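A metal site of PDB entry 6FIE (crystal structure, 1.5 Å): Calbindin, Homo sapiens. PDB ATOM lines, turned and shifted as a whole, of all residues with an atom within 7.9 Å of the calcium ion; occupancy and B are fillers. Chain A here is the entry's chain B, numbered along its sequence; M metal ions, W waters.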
ATOM      1  N   PHE A 198     -27.952 -10.267  31.377  1.00  0.00           N
ATOM      2  CA  PHE A 198     -27.220  -9.004  31.591  1.00  0.00           C
ATOM      3  C   PHE A 198     -25.807  -9.038  30.960  1.00  0.00           C
ATOM      4  O   PHE A 198     -25.399  -8.079  30.267  1.00  0.00           O
ATOM      5  CB  PHE A 198     -27.124  -8.722  33.104  1.00  0.00           C
ATOM      6  CG  PHE A 198     -26.566  -7.348  33.396  1.00  0.00           C
ATOM      7  CD1 PHE A 198     -27.387  -6.246  33.435  1.00  0.00           C
ATOM      8  CD2 PHE A 198     -25.194  -7.162  33.487  1.00  0.00           C
ATOM      9  CE1 PHE A 198     -26.842  -4.965  33.576  1.00  0.00           C
ATOM     10  CE2 PHE A 198     -24.667  -5.889  33.696  1.00  0.00           C
ATOM     11  CZ  PHE A 198     -25.498  -4.809  33.690  1.00  0.00           C
ATOM     12  N   TYR A 201     -26.073  -8.833  27.099  1.00  0.00           N
ATOM     13  CA  TYR A 201     -26.496  -7.535  26.550  1.00  0.00           C
ATOM     14  C   TYR A 201     -25.535  -6.415  26.927  1.00  0.00           C
ATOM     15  O   TYR A 201     -25.629  -5.364  26.311  1.00  0.00           O
ATOM     16  CB  TYR A 201     -27.974  -7.226  26.844  1.00  0.00           C
ATOM     17  CG  TYR A 201     -28.859  -8.147  26.033  1.00  0.00           C
ATOM     18  CD1 TYR A 201     -28.950  -8.007  24.644  1.00  0.00           C
ATOM     19  CD2 TYR A 201     -29.503  -9.225  26.614  1.00  0.00           C
ATOM     20  CE1 TYR A 201     -29.684  -8.901  23.879  1.00  0.00           C
ATOM     21  CE2 TYR A 201     -30.257 -10.121  25.863  1.00  0.00           C
ATOM     22  CZ  TYR A 201     -30.344  -9.956  24.490  1.00  0.00           C
ATOM     23  OH  TYR A 201     -31.097 -10.836  23.720  1.00  0.00           O
ATOM     24  N   ASP A 202     -24.562  -6.647  27.848  1.00  0.00           N
ATOM     25  CA  ASP A 202     -23.514  -5.631  28.097  1.00  0.00           C
ATOM     26  C   ASP A 202     -22.438  -5.938  27.061  1.00  0.00           C
ATOM     27  O   ASP A 202     -21.471  -6.611  27.342  1.00  0.00           O
ATOM     28  CB  ASP A 202     -22.973  -5.741  29.559  1.00  0.00           C
ATOM     29  CG  ASP A 202     -21.769  -4.845  29.799  1.00  0.00           C
ATOM     30  OD1 ASP A 202     -21.593  -3.873  29.047  1.00  0.00           O
ATOM     31  OD2 ASP A 202     -20.980  -5.138  30.744  1.00  0.00           O
ATOM     32  N   GLN A 203     -22.672  -5.534  25.822  1.00  0.00           N
ATOM     33  CA  GLN A 203     -21.841  -5.954  24.689  1.00  0.00           C
ATOM     34  C   GLN A 203     -20.413  -5.453  24.699  1.00  0.00           C
ATOM     35  O   GLN A 203     -19.513  -6.195  24.267  1.00  0.00           O
ATOM     36  CB  GLN A 203     -22.545  -5.604  23.388  1.00  0.00           C
ATOM     37  CG  GLN A 203     -23.968  -6.211  23.391  1.00  0.00           C
ATOM     38  CD  GLN A 203     -24.459  -6.738  22.075  1.00  0.00           C
ATOM     39  OE1 GLN A 203     -23.676  -7.228  21.251  1.00  0.00           O
ATOM     40  NE2 GLN A 203     -25.787  -6.749  21.919  1.00  0.00           N
ATOM     41  N   ASP A 204     -20.163  -4.244  25.211  1.00  0.00           N
ATOM     42  CA  ASP A 204     -18.815  -3.707  25.344  1.00  0.00           C
ATOM     43  C   ASP A 204     -18.114  -4.134  26.677  1.00  0.00           C
ATOM     44  O   ASP A 204     -16.954  -3.824  26.892  1.00  0.00           O
ATOM     45  CB  ASP A 204     -18.784  -2.209  25.126  1.00  0.00           C
ATOM     46  CG  ASP A 204     -19.621  -1.371  26.062  1.00  0.00           C
ATOM     47  OD1 ASP A 204     -20.076  -1.921  27.124  1.00  0.00           O
ATOM     48  OD2 ASP A 204     -19.785  -0.176  25.770  1.00  0.00           O
ATOM     49  N   GLY A 205     -18.834  -4.851  27.547  1.00  0.00           N
ATOM     50  CA  GLY A 205     -18.264  -5.439  28.757  1.00  0.00           C
ATOM     51  C   GLY A 205     -17.774  -4.466  29.793  1.00  0.00           C
ATOM     52  O   GLY A 205     -16.882  -4.813  30.574  1.00  0.00           O
ATOM     53  N   ASN A 206     -18.327  -3.237  29.813  1.00  0.00           N
ATOM     54  CA  ASN A 206     -17.931  -2.171  30.747  1.00  0.00           C
ATOM     55  C   ASN A 206     -18.695  -2.204  32.087  1.00  0.00           C
ATOM     56  O   ASN A 206     -18.449  -1.345  32.944  1.00  0.00           O
ATOM     57  CB  ASN A 206     -18.027  -0.786  30.094  1.00  0.00           C
ATOM     58  CG  ASN A 206     -19.387  -0.323  29.654  1.00  0.00           C
ATOM     59  OD1 ASN A 206     -20.394  -1.002  29.829  1.00  0.00           O
ATOM     60  ND2 ASN A 206     -19.462   0.884  29.151  1.00  0.00           N
ATOM     61  N   GLY A 207     -19.584  -3.193  32.265  1.00  0.00           N
ATOM     62  CA  GLY A 207     -20.271  -3.404  33.542  1.00  0.00           C
ATOM     63  C   GLY A 207     -21.683  -2.862  33.662  1.00  0.00           C
ATOM     64  O   GLY A 207     -22.357  -3.168  34.622  1.00  0.00           O
ATOM     65  N   TYR A 208     -22.154  -2.110  32.666  1.00  0.00           N
ATOM     66  CA  TYR A 208     -23.462  -1.565  32.669  1.00  0.00           C
ATOM     67  C   TYR A 208     -24.072  -1.597  31.281  1.00  0.00           C
ATOM     68  O   TYR A 208     -23.324  -1.642  30.294  1.00  0.00           O
ATOM     69  CB  TYR A 208     -23.490  -0.136  33.276  1.00  0.00           C
ATOM     70  CG  TYR A 208     -22.658   0.881  32.544  1.00  0.00           C
ATOM     71  CD1 TYR A 208     -23.144   1.525  31.417  1.00  0.00           C
ATOM     72  CD2 TYR A 208     -21.367   1.168  32.950  1.00  0.00           C
ATOM     73  CE1 TYR A 208     -22.400   2.492  30.768  1.00  0.00           C
ATOM     74  CE2 TYR A 208     -20.610   2.131  32.297  1.00  0.00           C
ATOM     75  CZ  TYR A 208     -21.121   2.777  31.192  1.00  0.00           C
ATOM     76  OH  TYR A 208     -20.408   3.763  30.579  1.00  0.00           O
ATOM     77  N   ILE A 209     -25.382  -1.497  31.233  1.00  0.00           N
ATOM     78  CA  ILE A 209     -26.126  -1.469  29.965  1.00  0.00           C
ATOM     79  C   ILE A 209     -26.487  -0.010  29.696  1.00  0.00           C
ATOM     80  O   ILE A 209     -27.141   0.652  30.528  1.00  0.00           O
ATOM     81  CB  ILE A 209     -27.330  -2.434  30.010  1.00  0.00           C
ATOM     82  CG1 ILE A 209     -26.775  -3.897  29.887  1.00  0.00           C
ATOM     83  CG2 ILE A 209     -28.385  -2.143  28.922  1.00  0.00           C
ATOM     84  CD1 ILE A 209     -27.757  -4.992  29.950  1.00  0.00           C
ATOM     85  N   ASP A 210     -26.091   0.498  28.510  1.00  0.00           N
ATOM     86  CA  ASP A 210     -26.410   1.843  28.070  1.00  0.00           C
ATOM     87  C   ASP A 210     -27.635   1.778  27.153  1.00  0.00           C
ATOM     88  O   ASP A 210     -28.168   0.700  26.906  1.00  0.00           O
ATOM     89  CB  ASP A 210     -25.196   2.502  27.420  1.00  0.00           C
ATOM     90  CG  ASP A 210     -24.662   1.850  26.179  1.00  0.00           C
ATOM     91  OD1 ASP A 210     -25.465   1.251  25.443  1.00  0.00           O
ATOM     92  OD2 ASP A 210     -23.452   2.034  25.891  1.00  0.00           O
ATOM     93  N   GLU A 211     -28.119   2.917  26.702  1.00  0.00           N
ATOM     94  CA  GLU A 211     -29.328   2.992  25.879  1.00  0.00           C
ATOM     95  C   GLU A 211     -29.272   2.193  24.576  1.00  0.00           C
ATOM     96  O   GLU A 211     -30.273   1.551  24.250  1.00  0.00           O
ATOM     97  CB  GLU A 211     -29.678   4.460  25.613  1.00  0.00           C
ATOM     98  CG  GLU A 211     -31.118   4.680  25.150  1.00  0.00           C
ATOM     99  CD  GLU A 211     -31.689   6.078  25.330  1.00  0.00           C
ATOM    100  OE1 GLU A 211     -30.990   6.961  25.874  1.00  0.00           O
ATOM    101  OE2 GLU A 211     -32.881   6.274  24.975  1.00  0.00           O
ATOM    102  N   GLU A 213     -27.330  -0.496  23.983  1.00  0.00           N
ATOM    103  CA  GLU A 213     -27.399  -1.877  24.423  1.00  0.00           C
ATOM    104  C   GLU A 213     -28.813  -2.262  24.906  1.00  0.00           C
ATOM    105  O   GLU A 213     -29.239  -3.382  24.649  1.00  0.00           O
ATOM    106  CB  GLU A 213     -26.422  -2.114  25.555  1.00  0.00           C
ATOM    107  CG  GLU A 213     -24.996  -2.137  25.121  1.00  0.00           C
ATOM    108  CD  GLU A 213     -24.032  -2.042  26.272  1.00  0.00           C
ATOM    109  OE1 GLU A 213     -24.348  -1.337  27.268  1.00  0.00           O
ATOM    110  OE2 GLU A 213     -22.898  -2.541  26.118  1.00  0.00           O
ATOM    111  N   LEU A 250     -27.434   1.479  33.273  1.00  0.00           N
ATOM    112  CA  LEU A 250     -28.244   0.489  33.933  1.00  0.00           C
ATOM    113  C   LEU A 250     -27.316  -0.565  34.455  1.00  0.00           C
ATOM    114  O   LEU A 250     -26.757  -1.362  33.703  1.00  0.00           O
ATOM    115  CB  LEU A 250     -29.285  -0.185  33.015  1.00  0.00           C
ATOM    116  CG  LEU A 250     -30.391   0.693  32.570  1.00  0.00           C
ATOM    117  CD1 LEU A 250     -30.969   0.180  31.225  1.00  0.00           C
ATOM    118  CD2 LEU A 250     -31.471   0.813  33.660  1.00  0.00           C
HETATM  119 CA    CA M   1     -22.031  -1.670  28.341  1.00  0.00          CA
HETATM  120  O   HOH W   1     -21.801   0.530  27.426  1.00  0.00           O
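OD2 of Asp 202 sits at hydrogen-bond distance from N of Gly 207, 2.8 Å away. The backbone NH (N) of Gln 203 lies close to the side-chain carboxylate (OE2) of Glu 213, 3.0 Å away. The side-chain carboxylate (OD1) of Asp 202 lies close to the backbone NH (N) of Gly 205 (3.3 Å). The side-chain carboxylate (OD1) of Asp 210 is in hydrogen-bond range of the backbone NH (N) of Glu 213.
Water W1 lies within hydrogen-bond range of OD2 of Asp 204 (2.7 Å), OD2 of Asp 210 (2.7 Å) and ND2 of Asn 206 (2.9 Å).
Within 4 Å of the calcium ion: Asp 202, Asp 204, Asn 206, Tyr 208 and Glu 213.
The calcium ion is bound by OD1 of Asn 206, 2.3 Å away. The side-chain carboxylate (OD1) of Asp 204 is bound to the calcium ion (2.3 Å). The backbone carbonyl oxygen (O) of Tyr 208 binds the calcium ion (2.3 Å). OD1 of Asp 202 is bound to the calcium ion (2.4 Å). Water W1 is bound to the calcium ion (2.4 Å). OE2 of Glu 213 binds the calcium ion, at 2.5 Å. The calcium ion is bound by OE1 of Glu 213, at 2.6 Å.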
